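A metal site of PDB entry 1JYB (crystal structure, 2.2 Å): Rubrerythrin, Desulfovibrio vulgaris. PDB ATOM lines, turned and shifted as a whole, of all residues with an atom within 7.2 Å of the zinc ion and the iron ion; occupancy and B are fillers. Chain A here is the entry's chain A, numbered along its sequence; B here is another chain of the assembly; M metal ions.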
ATOM      1  N   ALA A  16      27.162  -5.331  18.289  1.00  0.00           N
ATOM      2  CA  ALA A  16      26.352  -6.364  18.884  1.00  0.00           C
ATOM      3  C   ALA A  16      25.363  -6.849  17.816  1.00  0.00           C
ATOM      4  O   ALA A  16      25.279  -8.045  17.575  1.00  0.00           O
ATOM      5  CB  ALA A  16      25.659  -5.742  20.087  1.00  0.00           C
ATOM      6  N   GLY A  19      27.252  -9.221  15.373  1.00  0.00           N
ATOM      7  CA  GLY A  19      27.599 -10.477  15.945  1.00  0.00           C
ATOM      8  C   GLY A  19      26.330 -11.272  16.094  1.00  0.00           C
ATOM      9  O   GLY A  19      26.272 -12.460  15.780  1.00  0.00           O
ATOM     10  N   GLU A  20      25.219 -10.680  16.444  1.00  0.00           N
ATOM     11  CA  GLU A  20      24.002 -11.468  16.633  1.00  0.00           C
ATOM     12  C   GLU A  20      23.463 -11.973  15.311  1.00  0.00           C
ATOM     13  O   GLU A  20      22.811 -13.026  15.260  1.00  0.00           O
ATOM     14  CB  GLU A  20      22.932 -10.644  17.264  1.00  0.00           C
ATOM     15  CG  GLU A  20      23.330 -10.208  18.652  1.00  0.00           C
ATOM     16  CD  GLU A  20      23.245 -11.350  19.654  1.00  0.00           C
ATOM     17  OE1 GLU A  20      24.152 -12.261  19.677  1.00  0.00           O
ATOM     18  OE2 GLU A  20      22.271 -11.393  20.471  1.00  0.00           O
ATOM     19  N   ALA A  23      25.322 -14.985  14.481  1.00  0.00           N
ATOM     20  CA  ALA A  23      24.947 -16.099  15.374  1.00  0.00           C
ATOM     21  C   ALA A  23      23.637 -16.681  14.942  1.00  0.00           C
ATOM     22  O   ALA A  23      23.541 -17.910  14.924  1.00  0.00           O
ATOM     23  CB  ALA A  23      24.773 -15.690  16.866  1.00  0.00           C
ATOM     24  N   TYR A  27      23.573 -20.656  14.170  1.00  0.00           N
ATOM     25  CA  TYR A  27      22.666 -21.555  14.903  1.00  0.00           C
ATOM     26  C   TYR A  27      21.698 -22.202  13.929  1.00  0.00           C
ATOM     27  O   TYR A  27      21.365 -23.384  14.099  1.00  0.00           O
ATOM     28  CB  TYR A  27      21.869 -20.786  16.006  1.00  0.00           C
ATOM     29  CG  TYR A  27      22.743 -20.219  17.123  1.00  0.00           C
ATOM     30  CD1 TYR A  27      23.999 -20.763  17.407  1.00  0.00           C
ATOM     31  CD2 TYR A  27      22.281 -19.132  17.850  1.00  0.00           C
ATOM     32  CE1 TYR A  27      24.783 -20.222  18.409  1.00  0.00           C
ATOM     33  CE2 TYR A  27      23.062 -18.608  18.857  1.00  0.00           C
ATOM     34  CZ  TYR A  27      24.307 -19.148  19.112  1.00  0.00           C
ATOM     35  OH  TYR A  27      25.082 -18.576  20.114  1.00  0.00           O
ATOM     36  N   THR A  49      16.809 -20.798  19.286  1.00  0.00           N
ATOM     37  CA  THR A  49      17.838 -19.854  19.674  1.00  0.00           C
ATOM     38  C   THR A  49      18.192 -18.896  18.532  1.00  0.00           C
ATOM     39  O   THR A  49      18.404 -17.694  18.751  1.00  0.00           O
ATOM     40  CB  THR A  49      19.043 -20.660  20.091  1.00  0.00           C
ATOM     41  OG1 THR A  49      18.585 -21.595  21.061  1.00  0.00           O
ATOM     42  CG2 THR A  49      20.141 -19.807  20.727  1.00  0.00           C
ATOM     43  N   GLN A  52      15.656 -16.349  18.606  1.00  0.00           N
ATOM     44  CA  GLN A  52      15.736 -15.435  19.718  1.00  0.00           C
ATOM     45  C   GLN A  52      16.853 -14.467  19.418  1.00  0.00           C
ATOM     46  O   GLN A  52      16.708 -13.300  19.768  1.00  0.00           O
ATOM     47  CB  GLN A  52      15.990 -16.231  20.986  1.00  0.00           C
ATOM     48  CG  GLN A  52      14.666 -16.993  21.247  1.00  0.00           C
ATOM     49  CD  GLN A  52      14.732 -17.846  22.506  1.00  0.00           C
ATOM     50  OE1 GLN A  52      15.824 -18.276  22.898  1.00  0.00           O
ATOM     51  NE2 GLN A  52      13.641 -18.081  23.199  1.00  0.00           N
ATOM     52  N   GLU A  53      17.955 -14.883  18.767  1.00  0.00           N
ATOM     53  CA  GLU A  53      19.010 -13.966  18.331  1.00  0.00           C
ATOM     54  C   GLU A  53      18.502 -12.935  17.323  1.00  0.00           C
ATOM     55  O   GLU A  53      18.895 -11.774  17.404  1.00  0.00           O
ATOM     56  CB  GLU A  53      20.160 -14.732  17.720  1.00  0.00           C
ATOM     57  CG  GLU A  53      21.043 -15.646  18.610  1.00  0.00           C
ATOM     58  CD  GLU A  53      21.286 -15.235  20.059  1.00  0.00           C
ATOM     59  OE1 GLU A  53      21.667 -14.106  20.459  1.00  0.00           O
ATOM     60  OE2 GLU A  53      21.173 -16.138  20.919  1.00  0.00           O
ATOM     61  N   HIS A  56      16.894 -10.188  19.699  1.00  0.00           N
ATOM     62  CA  HIS A  56      17.815  -9.351  20.434  1.00  0.00           C
ATOM     63  C   HIS A  56      18.417  -8.357  19.425  1.00  0.00           C
ATOM     64  O   HIS A  56      18.592  -7.182  19.713  1.00  0.00           O
ATOM     65  CB  HIS A  56      18.961 -10.181  21.007  1.00  0.00           C
ATOM     66  CG  HIS A  56      18.591 -11.181  22.095  1.00  0.00           C
ATOM     67  ND1 HIS A  56      19.234 -12.314  22.369  1.00  0.00           N
ATOM     68  CD2 HIS A  56      17.537 -11.086  22.975  1.00  0.00           C
ATOM     69  CE1 HIS A  56      18.629 -12.904  23.371  1.00  0.00           C
ATOM     70  NE2 HIS A  56      17.616 -12.147  23.722  1.00  0.00           N
ATOM     71  N   SER A  90      29.050 -23.030  20.309  1.00  0.00           N
ATOM     72  CA  SER A  90      27.982 -22.092  20.555  1.00  0.00           C
ATOM     73  C   SER A  90      27.955 -21.725  22.017  1.00  0.00           C
ATOM     74  O   SER A  90      27.697 -20.555  22.296  1.00  0.00           O
ATOM     75  CB  SER A  90      26.635 -22.700  20.192  1.00  0.00           C
ATOM     76  OG  SER A  90      26.560 -23.070  18.823  1.00  0.00           O
ATOM     77  N   GLY A  93      30.599 -18.982  22.492  1.00  0.00           N
ATOM     78  CA  GLY A  93      30.190 -17.702  21.914  1.00  0.00           C
ATOM     79  C   GLY A  93      29.220 -17.052  22.869  1.00  0.00           C
ATOM     80  O   GLY A  93      29.382 -15.885  23.219  1.00  0.00           O
ATOM     81  N   GLU A  94      28.262 -17.831  23.372  1.00  0.00           N
ATOM     82  CA  GLU A  94      27.289 -17.392  24.376  1.00  0.00           C
ATOM     83  C   GLU A  94      27.968 -16.856  25.630  1.00  0.00           C
ATOM     84  O   GLU A  94      27.695 -15.772  26.135  1.00  0.00           O
ATOM     85  CB  GLU A  94      26.384 -18.544  24.763  1.00  0.00           C
ATOM     86  CG  GLU A  94      25.398 -18.991  23.665  1.00  0.00           C
ATOM     87  CD  GLU A  94      24.321 -17.972  23.241  1.00  0.00           C
ATOM     88  OE1 GLU A  94      24.193 -16.913  23.861  1.00  0.00           O
ATOM     89  OE2 GLU A  94      23.569 -18.250  22.300  1.00  0.00           O
ATOM     90  N   GLU A  97      29.601 -13.453  25.229  1.00  0.00           N
ATOM     91  CA  GLU A  97      28.616 -12.401  25.229  1.00  0.00           C
ATOM     92  C   GLU A  97      28.072 -11.962  26.568  1.00  0.00           C
ATOM     93  O   GLU A  97      27.993 -10.747  26.779  1.00  0.00           O
ATOM     94  CB  GLU A  97      27.429 -12.800  24.315  1.00  0.00           C
ATOM     95  CG  GLU A  97      27.757 -12.753  22.818  1.00  0.00           C
ATOM     96  CD  GLU A  97      26.565 -13.274  22.013  1.00  0.00           C
ATOM     97  OE1 GLU A  97      26.615 -14.107  21.104  1.00  0.00           O
ATOM     98  OE2 GLU A  97      25.405 -12.993  22.172  1.00  0.00           O
ATOM     99  N   MET A 101      31.326  -9.148  26.379  1.00  0.00           N
ATOM    100  CA  MET A 101      30.757  -8.132  25.499  1.00  0.00           C
ATOM    101  C   MET A 101      29.659  -7.292  26.076  1.00  0.00           C
ATOM    102  O   MET A 101      29.833  -6.074  26.219  1.00  0.00           O
ATOM    103  CB  MET A 101      30.234  -8.784  24.224  1.00  0.00           C
ATOM    104  CG  MET A 101      29.572  -7.897  23.164  1.00  0.00           C
ATOM    105  SD  MET A 101      28.990  -8.742  21.673  1.00  0.00           S
ATOM    106  CE  MET A 101      27.257  -8.720  21.978  1.00  0.00           C
ATOM    107  N   TYR A 102      28.527  -7.867  26.441  1.00  0.00           N
ATOM    108  CA  TYR A 102      27.408  -7.078  26.950  1.00  0.00           C
ATOM    109  C   TYR A 102      27.635  -6.353  28.248  1.00  0.00           C
ATOM    110  O   TYR A 102      27.115  -5.246  28.344  1.00  0.00           O
ATOM    111  CB  TYR A 102      26.131  -7.938  27.122  1.00  0.00           C
ATOM    112  CG  TYR A 102      25.423  -8.228  25.802  1.00  0.00           C
ATOM    113  CD1 TYR A 102      24.947  -7.191  25.026  1.00  0.00           C
ATOM    114  CD2 TYR A 102      25.292  -9.533  25.405  1.00  0.00           C
ATOM    115  CE1 TYR A 102      24.339  -7.452  23.832  1.00  0.00           C
ATOM    116  CE2 TYR A 102      24.697  -9.796  24.209  1.00  0.00           C
ATOM    117  CZ  TYR A 102      24.214  -8.767  23.441  1.00  0.00           C
ATOM    118  OH  TYR A 102      23.566  -9.098  22.261  1.00  0.00           O
ATOM    119  N   ILE A 124      19.681  -8.595  27.909  1.00  0.00           N
ATOM    120  CA  ILE A 124      19.949  -9.609  26.898  1.00  0.00           C
ATOM    121  C   ILE A 124      20.928 -10.591  27.481  1.00  0.00           C
ATOM    122  O   ILE A 124      20.829 -11.794  27.198  1.00  0.00           O
ATOM    123  CB  ILE A 124      20.493  -8.898  25.614  1.00  0.00           C
ATOM    124  CG1 ILE A 124      19.307  -8.335  24.853  1.00  0.00           C
ATOM    125  CG2 ILE A 124      21.203  -9.820  24.692  1.00  0.00           C
ATOM    126  CD1 ILE A 124      19.730  -7.293  23.805  1.00  0.00           C
ATOM    127  N   ALA A 127      19.407 -13.733  29.074  1.00  0.00           N
ATOM    128  CA  ALA A 127      19.000 -14.664  28.034  1.00  0.00           C
ATOM    129  C   ALA A 127      20.199 -15.386  27.485  1.00  0.00           C
ATOM    130  O   ALA A 127      20.139 -16.567  27.152  1.00  0.00           O
ATOM    131  CB  ALA A 127      18.329 -13.885  26.909  1.00  0.00           C
ATOM    132  N   GLU A 128      21.291 -14.674  27.253  1.00  0.00           N
ATOM    133  CA  GLU A 128      22.471 -15.318  26.764  1.00  0.00           C
ATOM    134  C   GLU A 128      23.054 -16.313  27.743  1.00  0.00           C
ATOM    135  O   GLU A 128      23.587 -17.321  27.256  1.00  0.00           O
ATOM    136  CB  GLU A 128      23.511 -14.271  26.392  1.00  0.00           C
ATOM    137  CG  GLU A 128      23.077 -13.254  25.319  1.00  0.00           C
ATOM    138  CD  GLU A 128      22.279 -13.682  24.102  1.00  0.00           C
ATOM    139  OE1 GLU A 128      22.135 -12.905  23.164  1.00  0.00           O
ATOM    140  OE2 GLU A 128      21.790 -14.806  23.927  1.00  0.00           O
ATOM    141  N   GLU A 129      22.906 -16.123  29.035  1.00  0.00           N
ATOM    142  CA  GLU A 129      23.301 -17.154  29.980  1.00  0.00           C
ATOM    143  C   GLU A 129      22.503 -18.465  29.924  1.00  0.00           C
ATOM    144  O   GLU A 129      23.091 -19.555  29.996  1.00  0.00           O
ATOM    145  CB  GLU A 129      23.231 -16.535  31.371  1.00  0.00           C
ATOM    146  CG  GLU A 129      23.721 -17.409  32.526  1.00  0.00           C
ATOM    147  CD  GLU A 129      24.054 -16.686  33.845  1.00  0.00           C
ATOM    148  OE1 GLU A 129      23.520 -15.601  34.104  1.00  0.00           O
ATOM    149  OE2 GLU A 129      24.853 -17.217  34.614  1.00  0.00           O
ATOM    150  N   PHE A 130      21.188 -18.446  29.719  1.00  0.00           N
ATOM    151  CA  PHE A 130      20.417 -19.669  29.678  1.00  0.00           C
ATOM    152  C   PHE A 130      20.689 -20.419  28.383  1.00  0.00           C
ATOM    153  O   PHE A 130      20.737 -21.651  28.360  1.00  0.00           O
ATOM    154  CB  PHE A 130      18.919 -19.326  29.882  1.00  0.00           C
ATOM    155  CG  PHE A 130      18.040 -20.587  29.851  1.00  0.00           C
ATOM    156  CD1 PHE A 130      18.319 -21.627  30.721  1.00  0.00           C
ATOM    157  CD2 PHE A 130      17.071 -20.758  28.883  1.00  0.00           C
ATOM    158  CE1 PHE A 130      17.636 -22.830  30.615  1.00  0.00           C
ATOM    159  CE2 PHE A 130      16.403 -21.967  28.783  1.00  0.00           C
ATOM    160  CZ  PHE A 130      16.680 -23.004  29.644  1.00  0.00           C
ATOM    161  N   HIS A 131      20.935 -19.698  27.313  1.00  0.00           N
ATOM    162  CA  HIS A 131      21.302 -20.340  26.063  1.00  0.00           C
ATOM    163  C   HIS A 131      22.584 -21.129  26.182  1.00  0.00           C
ATOM    164  O   HIS A 131      22.683 -22.254  25.681  1.00  0.00           O
ATOM    165  CB  HIS A 131      21.473 -19.301  24.956  1.00  0.00           C
ATOM    166  CG  HIS A 131      20.238 -18.552  24.471  1.00  0.00           C
ATOM    167  ND1 HIS A 131      20.480 -17.501  23.645  1.00  0.00           N
ATOM    168  CD2 HIS A 131      18.905 -18.776  24.665  1.00  0.00           C
ATOM    169  CE1 HIS A 131      19.225 -17.083  23.426  1.00  0.00           C
ATOM    170  NE2 HIS A 131      18.280 -17.820  24.004  1.00  0.00           N
ATOM    171  N   GLU A 132      23.633 -20.556  26.807  1.00  0.00           N
ATOM    172  CA  GLU A 132      24.880 -21.288  27.042  1.00  0.00           C
ATOM    173  C   GLU A 132      24.593 -22.501  27.915  1.00  0.00           C
ATOM    174  O   GLU A 132      25.027 -23.606  27.608  1.00  0.00           O
ATOM    175  CB  GLU A 132      25.861 -20.429  27.756  1.00  0.00           C
ATOM    176  CG  GLU A 132      27.091 -21.254  27.911  1.00  0.00           C
ATOM    177  CD  GLU A 132      27.942 -20.871  29.107  1.00  0.00           C
ATOM    178  OE1 GLU A 132      27.389 -20.525  30.154  1.00  0.00           O
ATOM    179  OE2 GLU A 132      29.166 -20.964  29.024  1.00  0.00           O
ATOM    180  N   PHE A 135      22.969 -25.311  25.760  1.00  0.00           N
ATOM    181  CA  PHE A 135      23.916 -25.948  24.832  1.00  0.00           C
ATOM    182  C   PHE A 135      24.906 -26.871  25.540  1.00  0.00           C
ATOM    183  O   PHE A 135      25.368 -27.915  25.027  1.00  0.00           O
ATOM    184  CB  PHE A 135      24.734 -24.885  24.077  1.00  0.00           C
ATOM    185  CG  PHE A 135      23.934 -24.036  23.104  1.00  0.00           C
ATOM    186  CD1 PHE A 135      22.961 -24.648  22.321  1.00  0.00           C
ATOM    187  CD2 PHE A 135      24.193 -22.673  23.022  1.00  0.00           C
ATOM    188  CE1 PHE A 135      22.254 -23.901  21.412  1.00  0.00           C
ATOM    189  CE2 PHE A 135      23.485 -21.922  22.103  1.00  0.00           C
ATOM    190  CZ  PHE A 135      22.534 -22.547  21.292  1.00  0.00           C
ATOM    191  N   CYS B 161      12.438 -13.742  23.386  1.00  0.00           N
ATOM    192  CA  CYS B 161      13.871 -13.530  23.327  1.00  0.00           C
ATOM    193  C   CYS B 161      14.671 -14.379  24.300  1.00  0.00           C
ATOM    194  O   CYS B 161      15.912 -14.304  24.300  1.00  0.00           O
ATOM    195  CB  CYS B 161      14.197 -12.079  23.583  1.00  0.00           C
ATOM    196  SG  CYS B 161      13.873 -11.639  25.322  1.00  0.00           S
HETATM  197 ZN    ZN M   1      23.511 -13.499  21.434  1.00  0.00          ZN
HETATM  198 FE    FE M   2      22.509 -16.491  22.683  1.00  0.00          FE
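Of the 24 residues printed, 4 come within 4 Å of the zinc ion.
The nearest printed residue that does not touch the zinc ion is Glu 94 (4.2 Å).
OE2 of Glu 97 binds the zinc ion.
The zinc ion is bound by OE1 of Glu 53 (2.2 Å).
OE1 of Glu 20 binds the zinc ion (2.2 Å).
OE1 of Glu 128 is bound to the zinc ion.
Slightly farther from the zinc ion lies the side-chain carboxylate (OE2) of Glu 20 (2.6 Å).
The side-chain carboxylate (OE2) of Glu 94 binds the iron ion.
The iron ion is bound by OE1 of Glu 94 (2.1 Å).
The iron ion is bound by OE2 of Glu 128 (2.2 Å).
The iron ion is bound by OE2 of Glu 53 (2.2 Å).
ND1 of His 131 is bound to the iron ion, 2.5 Å away.
The iron ion has five donor atoms within binding distance.
OH of Tyr 27 lies close to OE2 of Glu 94 (2.7 Å).
The backbone NH of Tyr 102 lies within hydrogen-bond range of the backbone carbonyl oxygen of Glu 97.
The side-chain carboxylate (OE1) of Glu 128 sits close to a ring nitrogen (ND1) of His 56, 3.1 Å away.
The side-chain hydroxyl (OH) of Tyr 102 is in hydrogen-bond range of the side-chain carboxylate (OE2) of Glu 20.
OE1 of Gln 52 sits at hydrogen-bond distance from NE2 of His 131 (2.7 Å).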
